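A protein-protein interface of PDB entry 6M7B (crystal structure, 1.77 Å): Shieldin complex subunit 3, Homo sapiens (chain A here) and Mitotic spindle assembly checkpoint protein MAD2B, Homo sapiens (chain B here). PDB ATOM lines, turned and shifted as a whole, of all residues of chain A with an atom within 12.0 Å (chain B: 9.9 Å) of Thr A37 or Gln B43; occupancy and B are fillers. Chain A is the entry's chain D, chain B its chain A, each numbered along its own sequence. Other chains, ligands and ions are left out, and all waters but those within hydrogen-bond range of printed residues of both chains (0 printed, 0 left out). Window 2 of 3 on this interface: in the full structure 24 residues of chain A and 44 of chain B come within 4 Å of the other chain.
O of Thr A37 is in hydrogen-bond range of NE2 of Gln B43, 2.9 Å away. SG of Cys B56 is in hydrogen-bond range of O of Leu A36 (3.6 Å).
The backbone carbonyl oxygen (O) of Ile B41 sits at hydrogen-bond distance from the backbone NH (N) of Cys B56, 2.7 Å away. NE of Arg B45 is in hydrogen-bond range of OE1 of Gln B43 (3.5 Å). O of Met B54 is in hydrogen-bond range of N of Gln B43 (2.8 Å). OG of Ser B55 sits at hydrogen-bond distance from N of His B57 (3.0 Å). The side-chain amide oxygen of Asn B61 sits close to the backbone carbonyl oxygen of His B57, 3.2 Å away. O of Val A32 sits at hydrogen-bond distance from N of Thr A37.
Pro B38 touches Ile A24. Ile A24 touches Ile B41 (CG2 to CG2, 3.9 Å). Glu A26 touches Pro B38 (OE2 to CB, 3.7 Å). Pro B38 touches Ala A29. Ile B41 touches Ala A29 (CG2 to CB, 3.7 Å). Val A32 touches Ile B41. Val A32 touches Cys B56 (CG1 to CB, 3.7 Å). CG2 of Val A32 touches ND1 of His B57 (3.9 Å). Lys A33 touches Gly B40. CG2 of Thr A37 touches SG of Cys B56, at 3.8 Å.
Of the printed residues of chain B, Val A32 touches Ile B41, Cys B56 and His B57. Of the printed residues of chain B, Lys A33 touches Gly B40. Printed residues of chain B within 4 Å of Leu A36: Cys B56 (3.4 Å). Of the printed residues of chain B, Thr A37 touches Gln B43 (2.9 Å) and Cys B56 (3.8 Å). Of chain A, only Ala A29 (3.9 Å) and Lys A33 (3.4 Å) come within 4 Å of Gly B40. Of chain A, only Ile A24, Ala A29 and Val A32 come within 4 Å of Ile B41. Of chain A, only Thr A37 comes within 4 Å of Gln B43. No residue of chain A comes within 4 Å of Lys B44. No residue of chain A comes within 4 Å of Val B52. No residue of chain A comes within 4 Å of Gln B53. No residue of chain A comes within 4 Å of Met B54. No residue of chain A comes within 4 Å of Ser B55. Of the printed residues of chain A, Cys B56 touches Val A32, Leu A36 and Thr A37. Printed residues of chain A within 4 Å of His B57: Ile A24 (3.5 Å) and Val A32 (3.9 Å). The nearest residue of chain B that does not touch Thr A37 is Phe B42 (4.2 Å). The nearest printed residue of chain B that does not touch Glu A26 is Val B39 (5.6 Å).
Printed residues of chain B that touch a printed residue of chain A: Pro B38, Gly B40, Ile B41, Gln B43, Cys B56 and His B57. Hydrophobic or aromatic side chains of chain B that line the printed part of chain A: Pro B38, Ile B41 and His B57. Of the 13 printed residues of chain A, 7 touch a printed residue of chain B. Hydrophobic or aromatic side chains of chain A within 4 Å of the printed part of chain B: Ile A24, Ala A29, Val A32 and Leu A36. Among the printed residues, 14 pairs touch across the chains. Among the printed residues, no Asp or Glu carboxylate lies within 4 Å of a Lys or Arg side-chain nitrogen of the other chain.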
ATOM      1  N   ILE A  24     -19.444 -33.394 -22.381  1.00  0.00           N
ATOM      2  CA  ILE A  24     -18.757 -32.209 -22.897  1.00  0.00           C
ATOM      3  C   ILE A  24     -18.947 -32.182 -24.406  1.00  0.00           C
ATOM      4  O   ILE A  24     -18.240 -32.885 -25.138  1.00  0.00           O
ATOM      5  CB  ILE A  24     -17.268 -32.194 -22.544  1.00  0.00           C
ATOM      6  CG1 ILE A  24     -17.077 -32.319 -21.033  1.00  0.00           C
ATOM      7  CG2 ILE A  24     -16.597 -30.941 -23.114  1.00  0.00           C
ATOM      8  CD1 ILE A  24     -15.613 -32.191 -20.596  1.00  0.00           C
ATOM      9  N   GLU A  26     -18.853 -30.517 -28.281  1.00  0.00           N
ATOM     10  CA  GLU A  26     -17.874 -29.715 -29.007  1.00  0.00           C
ATOM     11  C   GLU A  26     -18.076 -28.222 -28.755  1.00  0.00           C
ATOM     12  O   GLU A  26     -17.098 -27.464 -28.713  1.00  0.00           O
ATOM     13  CB  GLU A  26     -17.939 -30.027 -30.506  1.00  0.00           C
ATOM     14  CG  GLU A  26     -17.502 -31.446 -30.868  1.00  0.00           C
ATOM     15  CD  GLU A  26     -15.987 -31.589 -31.012  1.00  0.00           C
ATOM     16  OE1 GLU A  26     -15.298 -30.561 -31.205  1.00  0.00           O
ATOM     17  OE2 GLU A  26     -15.482 -32.733 -30.932  1.00  0.00           O
ATOM     18  N   GLU A  27     -19.324 -27.779 -28.570  1.00  0.00           N
ATOM     19  CA  GLU A  27     -19.554 -26.354 -28.351  1.00  0.00           C
ATOM     20  C   GLU A  27     -19.118 -25.942 -26.944  1.00  0.00           C
ATOM     21  O   GLU A  27     -18.485 -24.896 -26.763  1.00  0.00           O
ATOM     22  CB  GLU A  27     -21.025 -25.995 -28.609  1.00  0.00           C
ATOM     23  CG  GLU A  27     -21.996 -26.258 -27.476  1.00  0.00           C
ATOM     24  CD  GLU A  27     -22.197 -25.036 -26.582  1.00  0.00           C
ATOM     25  OE1 GLU A  27     -21.913 -23.907 -27.032  1.00  0.00           O
ATOM     26  OE2 GLU A  27     -22.623 -25.206 -25.422  1.00  0.00           O
ATOM     27  N   ALA A  28     -19.427 -26.760 -25.931  1.00  0.00           N
ATOM     28  CA  ALA A  28     -18.903 -26.503 -24.595  1.00  0.00           C
ATOM     29  C   ALA A  28     -17.387 -26.476 -24.611  1.00  0.00           C
ATOM     30  O   ALA A  28     -16.767 -25.648 -23.939  1.00  0.00           O
ATOM     31  CB  ALA A  28     -19.397 -27.569 -23.614  1.00  0.00           C
ATOM     32  N   ALA A  29     -16.770 -27.399 -25.355  1.00  0.00           N
ATOM     33  CA  ALA A  29     -15.319 -27.393 -25.461  1.00  0.00           C
ATOM     34  C   ALA A  29     -14.821 -26.115 -26.120  1.00  0.00           C
ATOM     35  O   ALA A  29     -13.739 -25.621 -25.773  1.00  0.00           O
ATOM     36  CB  ALA A  29     -14.841 -28.625 -26.236  1.00  0.00           C
ATOM     37  N   GLU A  30     -15.588 -25.566 -27.074  1.00  0.00           N
ATOM     38  CA  GLU A  30     -15.175 -24.315 -27.697  1.00  0.00           C
ATOM     39  C   GLU A  30     -15.172 -23.180 -26.682  1.00  0.00           C
ATOM     40  O   GLU A  30     -14.297 -22.308 -26.731  1.00  0.00           O
ATOM     41  CB  GLU A  30     -16.084 -23.986 -28.886  1.00  0.00           C
ATOM     42  CG  GLU A  30     -15.610 -22.782 -29.714  1.00  0.00           C
ATOM     43  CD  GLU A  30     -16.654 -22.287 -30.716  1.00  0.00           C
ATOM     44  OE1 GLU A  30     -16.482 -21.172 -31.257  1.00  0.00           O
ATOM     45  OE2 GLU A  30     -17.642 -23.011 -30.971  1.00  0.00           O
ATOM     46  N   ASP A  31     -16.123 -23.189 -25.741  1.00  0.00           N
ATOM     47  CA  ASP A  31     -16.141 -22.164 -24.703  1.00  0.00           C
ATOM     48  C   ASP A  31     -14.981 -22.343 -23.740  1.00  0.00           C
ATOM     49  O   ASP A  31     -14.364 -21.358 -23.315  1.00  0.00           O
ATOM     50  CB  ASP A  31     -17.470 -22.192 -23.951  1.00  0.00           C
ATOM     51  CG  ASP A  31     -18.609 -21.633 -24.773  1.00  0.00           C
ATOM     52  OD1 ASP A  31     -18.341 -20.798 -25.662  1.00  0.00           O
ATOM     53  OD2 ASP A  31     -19.767 -22.037 -24.541  1.00  0.00           O
ATOM     54  N   VAL A  32     -14.669 -23.596 -23.385  1.00  0.00           N
ATOM     55  CA  VAL A  32     -13.484 -23.861 -22.576  1.00  0.00           C
ATOM     56  C   VAL A  32     -12.238 -23.327 -23.272  1.00  0.00           C
ATOM     57  O   VAL A  32     -11.418 -22.628 -22.664  1.00  0.00           O
ATOM     58  CB  VAL A  32     -13.349 -25.365 -22.271  1.00  0.00           C
ATOM     59  CG1 VAL A  32     -12.069 -25.605 -21.499  1.00  0.00           C
ATOM     60  CG2 VAL A  32     -14.556 -25.871 -21.481  1.00  0.00           C
ATOM     61  N   LYS A  33     -12.074 -23.652 -24.556  1.00  0.00           N
ATOM     62  CA  LYS A  33     -10.889 -23.203 -25.283  1.00  0.00           C
ATOM     63  C   LYS A  33     -10.790 -21.683 -25.272  1.00  0.00           C
ATOM     64  O   LYS A  33      -9.739 -21.119 -24.947  1.00  0.00           O
ATOM     65  CB  LYS A  33     -10.923 -23.721 -26.720  1.00  0.00           C
ATOM     66  CG  LYS A  33      -9.791 -23.188 -27.584  1.00  0.00           C
ATOM     67  CD  LYS A  33      -9.644 -24.004 -28.858  1.00  0.00           C
ATOM     68  CE  LYS A  33      -8.368 -23.648 -29.600  1.00  0.00           C
ATOM     69  NZ  LYS A  33      -8.573 -23.754 -31.074  1.00  0.00           N
ATOM     70  N   GLN A  34     -11.894 -21.005 -25.594  1.00  0.00           N
ATOM     71  CA  GLN A  34     -11.850 -19.556 -25.781  1.00  0.00           C
ATOM     72  C   GLN A  34     -11.582 -18.819 -24.475  1.00  0.00           C
ATOM     73  O   GLN A  34     -10.883 -17.798 -24.464  1.00  0.00           O
ATOM     74  CB  GLN A  34     -13.160 -19.077 -26.405  1.00  0.00           C
ATOM     75  CG  GLN A  34     -13.237 -17.574 -26.585  1.00  0.00           C
ATOM     76  CD  GLN A  34     -14.590 -17.121 -27.093  1.00  0.00           C
ATOM     77  OE1 GLN A  34     -15.024 -16.000 -26.825  1.00  0.00           O
ATOM     78  NE2 GLN A  34     -15.268 -17.993 -27.829  1.00  0.00           N
ATOM     79  N   TYR A  35     -12.132 -19.306 -23.364  1.00  0.00           N
ATOM     80  CA  TYR A  35     -12.115 -18.547 -22.121  1.00  0.00           C
ATOM     81  C   TYR A  35     -11.149 -19.069 -21.072  1.00  0.00           C
ATOM     82  O   TYR A  35     -10.609 -18.266 -20.305  1.00  0.00           O
ATOM     83  CB  TYR A  35     -13.522 -18.503 -21.515  1.00  0.00           C
ATOM     84  CG  TYR A  35     -14.494 -17.676 -22.319  1.00  0.00           C
ATOM     85  CD1 TYR A  35     -14.440 -16.287 -22.291  1.00  0.00           C
ATOM     86  CD2 TYR A  35     -15.463 -18.278 -23.109  1.00  0.00           C
ATOM     87  CE1 TYR A  35     -15.329 -15.523 -23.026  1.00  0.00           C
ATOM     88  CE2 TYR A  35     -16.352 -17.528 -23.848  1.00  0.00           C
ATOM     89  CZ  TYR A  35     -16.283 -16.149 -23.804  1.00  0.00           C
ATOM     90  OH  TYR A  35     -17.170 -15.394 -24.538  1.00  0.00           O
ATOM     91  N   LEU A  36     -10.901 -20.379 -21.020  1.00  0.00           N
ATOM     92  CA  LEU A  36     -10.147 -20.983 -19.926  1.00  0.00           C
ATOM     93  C   LEU A  36      -8.788 -21.532 -20.346  1.00  0.00           C
ATOM     94  O   LEU A  36      -8.120 -22.180 -19.532  1.00  0.00           O
ATOM     95  CB  LEU A  36     -10.970 -22.095 -19.270  1.00  0.00           C
ATOM     96  CG  LEU A  36     -12.375 -21.722 -18.809  1.00  0.00           C
ATOM     97  CD1 LEU A  36     -13.123 -22.931 -18.245  1.00  0.00           C
ATOM     98  CD2 LEU A  36     -12.310 -20.609 -17.774  1.00  0.00           C
ATOM     99  N   THR A  37      -8.362 -21.319 -21.584  1.00  0.00           N
ATOM    100  CA  THR A  37      -7.019 -21.756 -21.956  1.00  0.00           C
ATOM    101  C   THR A  37      -6.137 -20.540 -22.235  1.00  0.00           C
ATOM    102  O   THR A  37      -4.931 -20.565 -21.977  1.00  0.00           O
ATOM    103  CB  THR A  37      -7.023 -22.705 -23.182  1.00  0.00           C
ATOM    104  OG1 THR A  37      -7.751 -22.110 -24.263  1.00  0.00           O
ATOM    105  CG2 THR A  37      -7.656 -24.032 -22.825  1.00  0.00           C
ATOM    106  OXT THR A  37      -6.612 -19.502 -22.696  1.00  0.00           O
ATOM    107  N   VAL B  25      -2.530 -36.812 -13.284  1.00  0.00           N
ATOM    108  CA  VAL B  25      -1.961 -36.378 -14.560  1.00  0.00           C
ATOM    109  C   VAL B  25      -2.176 -37.460 -15.624  1.00  0.00           C
ATOM    110  O   VAL B  25      -2.502 -37.167 -16.783  1.00  0.00           O
ATOM    111  CB  VAL B  25      -0.471 -36.022 -14.381  1.00  0.00           C
ATOM    112  CG1 VAL B  25       0.204 -35.804 -15.718  1.00  0.00           C
ATOM    113  CG2 VAL B  25      -0.315 -34.799 -13.457  1.00  0.00           C
ATOM    114  N   HIS B  28      -5.809 -37.421 -17.050  1.00  0.00           N
ATOM    115  CA  HIS B  28      -5.954 -36.325 -18.014  1.00  0.00           C
ATOM    116  C   HIS B  28      -5.302 -36.667 -19.353  1.00  0.00           C
ATOM    117  O   HIS B  28      -5.880 -36.444 -20.424  1.00  0.00           O
ATOM    118  CB  HIS B  28      -5.334 -35.042 -17.462  1.00  0.00           C
ATOM    119  CG  HIS B  28      -6.185 -34.338 -16.450  1.00  0.00           C
ATOM    120  ND1 HIS B  28      -6.871 -33.174 -16.740  1.00  0.00           N
ATOM    121  CD2 HIS B  28      -6.431 -34.608 -15.145  1.00  0.00           C
ATOM    122  CE1 HIS B  28      -7.521 -32.768 -15.658  1.00  0.00           C
ATOM    123  NE2 HIS B  28      -7.273 -33.624 -14.677  1.00  0.00           N
ATOM    124  N   LEU B  29      -4.079 -37.196 -19.310  1.00  0.00           N
ATOM    125  CA  LEU B  29      -3.363 -37.441 -20.557  1.00  0.00           C
ATOM    126  C   LEU B  29      -4.015 -38.562 -21.359  1.00  0.00           C
ATOM    127  O   LEU B  29      -4.119 -38.466 -22.591  1.00  0.00           O
ATOM    128  CB  LEU B  29      -1.896 -37.745 -20.262  1.00  0.00           C
ATOM    129  CG  LEU B  29      -0.977 -37.886 -21.468  1.00  0.00           C
ATOM    130  CD1 LEU B  29      -1.031 -36.630 -22.351  1.00  0.00           C
ATOM    131  CD2 LEU B  29       0.466 -38.165 -20.977  1.00  0.00           C
ATOM    132  N   TYR B  32      -6.909 -37.262 -23.306  1.00  0.00           N
ATOM    133  CA  TYR B  32      -6.482 -36.458 -24.449  1.00  0.00           C
ATOM    134  C   TYR B  32      -5.977 -37.351 -25.579  1.00  0.00           C
ATOM    135  O   TYR B  32      -6.413 -37.235 -26.733  1.00  0.00           O
ATOM    136  CB  TYR B  32      -5.397 -35.472 -23.998  1.00  0.00           C
ATOM    137  CG  TYR B  32      -4.667 -34.841 -25.156  1.00  0.00           C
ATOM    138  CD1 TYR B  32      -5.200 -33.747 -25.813  1.00  0.00           C
ATOM    139  CD2 TYR B  32      -3.469 -35.388 -25.632  1.00  0.00           C
ATOM    140  CE1 TYR B  32      -4.547 -33.175 -26.902  1.00  0.00           C
ATOM    141  CE2 TYR B  32      -2.815 -34.823 -26.722  1.00  0.00           C
ATOM    142  CZ  TYR B  32      -3.365 -33.721 -27.347  1.00  0.00           C
ATOM    143  OH  TYR B  32      -2.730 -33.149 -28.423  1.00  0.00           O
ATOM    144  N   PRO B  38     -13.396 -33.681 -26.577  1.00  0.00           N
ATOM    145  CA  PRO B  38     -12.857 -32.792 -27.618  1.00  0.00           C
ATOM    146  C   PRO B  38     -11.517 -32.182 -27.214  1.00  0.00           C
ATOM    147  O   PRO B  38     -11.305 -31.835 -26.050  1.00  0.00           O
ATOM    148  CB  PRO B  38     -13.942 -31.718 -27.758  1.00  0.00           C
ATOM    149  CG  PRO B  38     -15.185 -32.333 -27.233  1.00  0.00           C
ATOM    150  CD  PRO B  38     -14.752 -33.280 -26.147  1.00  0.00           C
ATOM    151  N   VAL B  39     -10.611 -32.044 -28.197  1.00  0.00           N
ATOM    152  CA  VAL B  39      -9.258 -31.553 -27.916  1.00  0.00           C
ATOM    153  C   VAL B  39      -9.300 -30.156 -27.324  1.00  0.00           C
ATOM    154  O   VAL B  39      -8.384 -29.752 -26.601  1.00  0.00           O
ATOM    155  CB  VAL B  39      -8.365 -31.553 -29.185  1.00  0.00           C
ATOM    156  CG1 VAL B  39      -8.225 -32.930 -29.769  1.00  0.00           C
ATOM    157  CG2 VAL B  39      -8.896 -30.563 -30.238  1.00  0.00           C
ATOM    158  N   GLY B  40     -10.347 -29.391 -27.633  1.00  0.00           N
ATOM    159  CA  GLY B  40     -10.394 -27.998 -27.236  1.00  0.00           C
ATOM    160  C   GLY B  40     -10.340 -27.769 -25.741  1.00  0.00           C
ATOM    161  O   GLY B  40     -10.009 -26.662 -25.312  1.00  0.00           O
ATOM    162  N   ILE B  41     -10.661 -28.780 -24.925  1.00  0.00           N
ATOM    163  CA  ILE B  41     -10.641 -28.542 -23.482  1.00  0.00           C
ATOM    164  C   ILE B  41      -9.250 -28.640 -22.878  1.00  0.00           C
ATOM    165  O   ILE B  41      -9.075 -28.286 -21.702  1.00  0.00           O
ATOM    166  CB  ILE B  41     -11.554 -29.496 -22.680  1.00  0.00           C
ATOM    167  CG1 ILE B  41     -11.058 -30.945 -22.743  1.00  0.00           C
ATOM    168  CG2 ILE B  41     -13.000 -29.411 -23.158  1.00  0.00           C
ATOM    169  CD1 ILE B  41     -11.837 -31.872 -21.790  1.00  0.00           C
ATOM    170  N   PHE B  42      -8.253 -29.111 -23.627  1.00  0.00           N
ATOM    171  CA  PHE B  42      -6.953 -29.426 -23.048  1.00  0.00           C
ATOM    172  C   PHE B  42      -5.965 -28.287 -23.241  1.00  0.00           C
ATOM    173  O   PHE B  42      -6.001 -27.577 -24.246  1.00  0.00           O
ATOM    174  CB  PHE B  42      -6.379 -30.704 -23.657  1.00  0.00           C
ATOM    175  CG  PHE B  42      -7.151 -31.928 -23.280  1.00  0.00           C
ATOM    176  CD1 PHE B  42      -6.902 -32.572 -22.078  1.00  0.00           C
ATOM    177  CD2 PHE B  42      -8.169 -32.393 -24.098  1.00  0.00           C
ATOM    178  CE1 PHE B  42      -7.637 -33.695 -21.712  1.00  0.00           C
ATOM    179  CE2 PHE B  42      -8.909 -33.518 -23.737  1.00  0.00           C
ATOM    180  CZ  PHE B  42      -8.645 -34.161 -22.541  1.00  0.00           C
ATOM    181  N   GLN B  43      -5.085 -28.121 -22.258  1.00  0.00           N
ATOM    182  CA  GLN B  43      -4.020 -27.127 -22.302  1.00  0.00           C
ATOM    183  C   GLN B  43      -2.717 -27.786 -21.881  1.00  0.00           C
ATOM    184  O   GLN B  43      -2.698 -28.601 -20.958  1.00  0.00           O
ATOM    185  CB  GLN B  43      -4.332 -25.938 -21.385  1.00  0.00           C
ATOM    186  CG  GLN B  43      -3.154 -25.028 -21.082  1.00  0.00           C
ATOM    187  CD  GLN B  43      -3.513 -23.981 -20.046  1.00  0.00           C
ATOM    188  OE1 GLN B  43      -3.604 -24.281 -18.850  1.00  0.00           O
ATOM    189  NE2 GLN B  43      -3.743 -22.750 -20.499  1.00  0.00           N
ATOM    190  N   LYS B  44      -1.632 -27.436 -22.565  1.00  0.00           N
ATOM    191  CA  LYS B  44      -0.341 -28.041 -22.269  1.00  0.00           C
ATOM    192  C   LYS B  44       0.181 -27.505 -20.945  1.00  0.00           C
ATOM    193  O   LYS B  44       0.187 -26.291 -20.712  1.00  0.00           O
ATOM    194  CB  LYS B  44       0.650 -27.748 -23.397  1.00  0.00           C
ATOM    195  CG  LYS B  44       1.418 -28.969 -23.902  1.00  0.00           C
ATOM    196  CD  LYS B  44       2.021 -28.700 -25.279  1.00  0.00           C
ATOM    197  CE  LYS B  44       2.875 -29.865 -25.763  1.00  0.00           C
ATOM    198  NZ  LYS B  44       2.150 -31.168 -25.698  1.00  0.00           N
ATOM    199  N   ARG B  45       0.579 -28.411 -20.057  1.00  0.00           N
ATOM    200  CA  ARG B  45       1.228 -28.038 -18.809  1.00  0.00           C
ATOM    201  C   ARG B  45       2.500 -28.855 -18.639  1.00  0.00           C
ATOM    202  O   ARG B  45       2.780 -29.779 -19.408  1.00  0.00           O
ATOM    203  CB  ARG B  45       0.307 -28.242 -17.608  1.00  0.00           C
ATOM    204  CG  ARG B  45      -0.752 -27.181 -17.486  1.00  0.00           C
ATOM    205  CD  ARG B  45      -1.734 -27.563 -16.422  1.00  0.00           C
ATOM    206  NE  ARG B  45      -3.012 -26.881 -16.589  1.00  0.00           N
ATOM    207  CZ  ARG B  45      -4.140 -27.294 -16.028  1.00  0.00           C
ATOM    208  NH1 ARG B  45      -5.270 -26.627 -16.225  1.00  0.00           N
ATOM    209  NH2 ARG B  45      -4.132 -28.382 -15.267  1.00  0.00           N
ATOM    210  N   LYS B  46       3.287 -28.492 -17.633  1.00  0.00           N
ATOM    211  CA  LYS B  46       4.505 -29.218 -17.310  1.00  0.00           C
ATOM    212  C   LYS B  46       4.291 -29.980 -16.011  1.00  0.00           C
ATOM    213  O   LYS B  46       3.949 -29.384 -14.985  1.00  0.00           O
ATOM    214  CB  LYS B  46       5.700 -28.269 -17.199  1.00  0.00           C
ATOM    215  CG  LYS B  46       7.033 -28.944 -17.451  1.00  0.00           C
ATOM    216  CD  LYS B  46       7.549 -28.667 -18.857  1.00  0.00           C
ATOM    217  CE  LYS B  46       8.271 -27.327 -18.948  1.00  0.00           C
ATOM    218  NZ  LYS B  46       8.757 -27.034 -20.334  1.00  0.00           N
ATOM    219  N   LYS B  47       4.462 -31.300 -16.069  1.00  0.00           N
ATOM    220  CA  LYS B  47       4.438 -32.168 -14.903  1.00  0.00           C
ATOM    221  C   LYS B  47       5.561 -33.176 -15.074  1.00  0.00           C
ATOM    222  O   LYS B  47       5.756 -33.694 -16.175  1.00  0.00           O
ATOM    223  CB  LYS B  47       3.091 -32.899 -14.754  1.00  0.00           C
ATOM    224  CG  LYS B  47       1.858 -31.989 -14.797  1.00  0.00           C
ATOM    225  CD  LYS B  47       1.544 -31.384 -13.430  1.00  0.00           C
ATOM    226  CE  LYS B  47       0.230 -30.610 -13.451  1.00  0.00           C
ATOM    227  NZ  LYS B  47      -0.118 -30.127 -12.084  1.00  0.00           N
ATOM    228  N   VAL B  50       7.845 -32.743 -17.868  1.00  0.00           N
ATOM    229  CA  VAL B  50       7.378 -33.278 -19.142  1.00  0.00           C
ATOM    230  C   VAL B  50       6.149 -32.493 -19.581  1.00  0.00           C
ATOM    231  O   VAL B  50       5.309 -32.142 -18.738  1.00  0.00           O
ATOM    232  CB  VAL B  50       7.078 -34.781 -19.009  1.00  0.00           C
ATOM    233  CG1 VAL B  50       6.087 -35.244 -20.048  1.00  0.00           C
ATOM    234  CG2 VAL B  50       8.374 -35.566 -19.090  1.00  0.00           C
ATOM    235  N   PRO B  51       6.001 -32.179 -20.871  1.00  0.00           N
ATOM    236  CA  PRO B  51       4.806 -31.453 -21.323  1.00  0.00           C
ATOM    237  C   PRO B  51       3.614 -32.398 -21.395  1.00  0.00           C
ATOM    238  O   PRO B  51       3.616 -33.363 -22.162  1.00  0.00           O
ATOM    239  CB  PRO B  51       5.207 -30.932 -22.711  1.00  0.00           C
ATOM    240  CG  PRO B  51       6.707 -31.170 -22.815  1.00  0.00           C
ATOM    241  CD  PRO B  51       6.960 -32.375 -21.971  1.00  0.00           C
ATOM    242  N   VAL B  52       2.604 -32.128 -20.569  1.00  0.00           N
ATOM    243  CA  VAL B  52       1.388 -32.931 -20.492  1.00  0.00           C
ATOM    244  C   VAL B  52       0.212 -32.068 -20.929  1.00  0.00           C
ATOM    245  O   VAL B  52       0.262 -30.840 -20.872  1.00  0.00           O
ATOM    246  CB  VAL B  52       1.162 -33.462 -19.072  1.00  0.00           C
ATOM    247  CG1 VAL B  52       2.370 -34.248 -18.625  1.00  0.00           C
ATOM    248  CG2 VAL B  52       0.927 -32.288 -18.138  1.00  0.00           C
ATOM    249  N   GLN B  53      -0.851 -32.726 -21.381  1.00  0.00           N
ATOM    250  CA  GLN B  53      -2.097 -32.053 -21.709  1.00  0.00           C
ATOM    251  C   GLN B  53      -3.072 -32.280 -20.563  1.00  0.00           C
ATOM    252  O   GLN B  53      -3.266 -33.423 -20.135  1.00  0.00           O
ATOM    253  CB  GLN B  53      -2.679 -32.581 -23.022  1.00  0.00           C
ATOM    254  CG  GLN B  53      -1.823 -32.273 -24.243  1.00  0.00           C
ATOM    255  CD  GLN B  53      -2.143 -30.925 -24.853  1.00  0.00           C
ATOM    256  OE1 GLN B  53      -2.919 -30.140 -24.302  1.00  0.00           O
ATOM    257  NE2 GLN B  53      -1.555 -30.651 -26.011  1.00  0.00           N
ATOM    258  N   MET B  54      -3.653 -31.195 -20.047  1.00  0.00           N
ATOM    259  CA  MET B  54      -4.577 -31.270 -18.919  1.00  0.00           C
ATOM    260  C   MET B  54      -5.883 -30.568 -19.283  1.00  0.00           C
ATOM    261  O   MET B  54      -5.872 -29.513 -19.937  1.00  0.00           O
ATOM    262  CB  MET B  54      -4.013 -30.577 -17.654  1.00  0.00           C
ATOM    263  CG  MET B  54      -2.641 -31.022 -17.120  1.00  0.00           C
ATOM    264  SD  MET B  54      -2.630 -32.313 -15.898  1.00  0.00           S
ATOM    265  CE  MET B  54      -3.696 -31.629 -14.626  1.00  0.00           C
ATOM    266  N   SER B  55      -6.998 -31.120 -18.812  1.00  0.00           N
ATOM    267  CA  SER B  55      -8.303 -30.517 -19.056  1.00  0.00           C
ATOM    268  C   SER B  55      -8.427 -29.177 -18.341  1.00  0.00           C
ATOM    269  O   SER B  55      -7.933 -28.996 -17.222  1.00  0.00           O
ATOM    270  CB  SER B  55      -9.407 -31.474 -18.587  1.00  0.00           C
ATOM    271  OG  SER B  55     -10.561 -30.776 -18.139  1.00  0.00           O
ATOM    272  N   CYS B  56      -9.094 -28.229 -18.996  1.00  0.00           N
ATOM    273  CA  CYS B  56      -9.475 -26.965 -18.386  1.00  0.00           C
ATOM    274  C   CYS B  56     -10.964 -26.920 -18.071  1.00  0.00           C
ATOM    275  O   CYS B  56     -11.477 -25.871 -17.676  1.00  0.00           O
ATOM    276  CB  CYS B  56      -9.093 -25.814 -19.310  1.00  0.00           C
ATOM    277  SG  CYS B  56      -7.295 -25.661 -19.356  1.00  0.00           S
ATOM    278  N   HIS B  57     -11.663 -28.026 -18.272  1.00  0.00           N
ATOM    279  CA  HIS B  57     -13.094 -28.107 -17.982  1.00  0.00           C
ATOM    280  C   HIS B  57     -13.292 -28.302 -16.487  1.00  0.00           C
ATOM    281  O   HIS B  57     -12.813 -29.300 -15.934  1.00  0.00           O
ATOM    282  CB  HIS B  57     -13.722 -29.269 -18.749  1.00  0.00           C
ATOM    283  CG  HIS B  57     -15.207 -29.370 -18.582  1.00  0.00           C
ATOM    284  ND1 HIS B  57     -16.099 -28.833 -19.489  1.00  0.00           N
ATOM    285  CD2 HIS B  57     -15.955 -29.940 -17.611  1.00  0.00           C
ATOM    286  CE1 HIS B  57     -17.334 -29.057 -19.076  1.00  0.00           C
ATOM    287  NE2 HIS B  57     -17.276 -29.733 -17.942  1.00  0.00           N
ATOM    288  N   PRO B  58     -13.962 -27.383 -15.796  1.00  0.00           N
ATOM    289  CA  PRO B  58     -13.957 -27.456 -14.322  1.00  0.00           C
ATOM    290  C   PRO B  58     -14.634 -28.699 -13.767  1.00  0.00           C
ATOM    291  O   PRO B  58     -14.101 -29.321 -12.840  1.00  0.00           O
ATOM    292  CB  PRO B  58     -14.689 -26.167 -13.903  1.00  0.00           C
ATOM    293  CG  PRO B  58     -14.656 -25.285 -15.099  1.00  0.00           C
ATOM    294  CD  PRO B  58     -14.638 -26.176 -16.297  1.00  0.00           C
ATOM    295  N   ASN B  61     -12.414 -31.738 -14.237  1.00  0.00           N
ATOM    296  CA  ASN B  61     -11.279 -31.680 -13.323  1.00  0.00           C
ATOM    297  C   ASN B  61     -11.680 -32.084 -11.917  1.00  0.00           C
ATOM    298  O   ASN B  61     -10.950 -32.828 -11.246  1.00  0.00           O
ATOM    299  CB  ASN B  61     -10.706 -30.274 -13.320  1.00  0.00           C
ATOM    300  CG  ASN B  61     -10.039 -29.940 -14.632  1.00  0.00           C
ATOM    301  OD1 ASN B  61      -9.982 -30.764 -15.532  1.00  0.00           O
ATOM    302  ND2 ASN B  61      -9.565 -28.713 -14.754  1.00  0.00           N
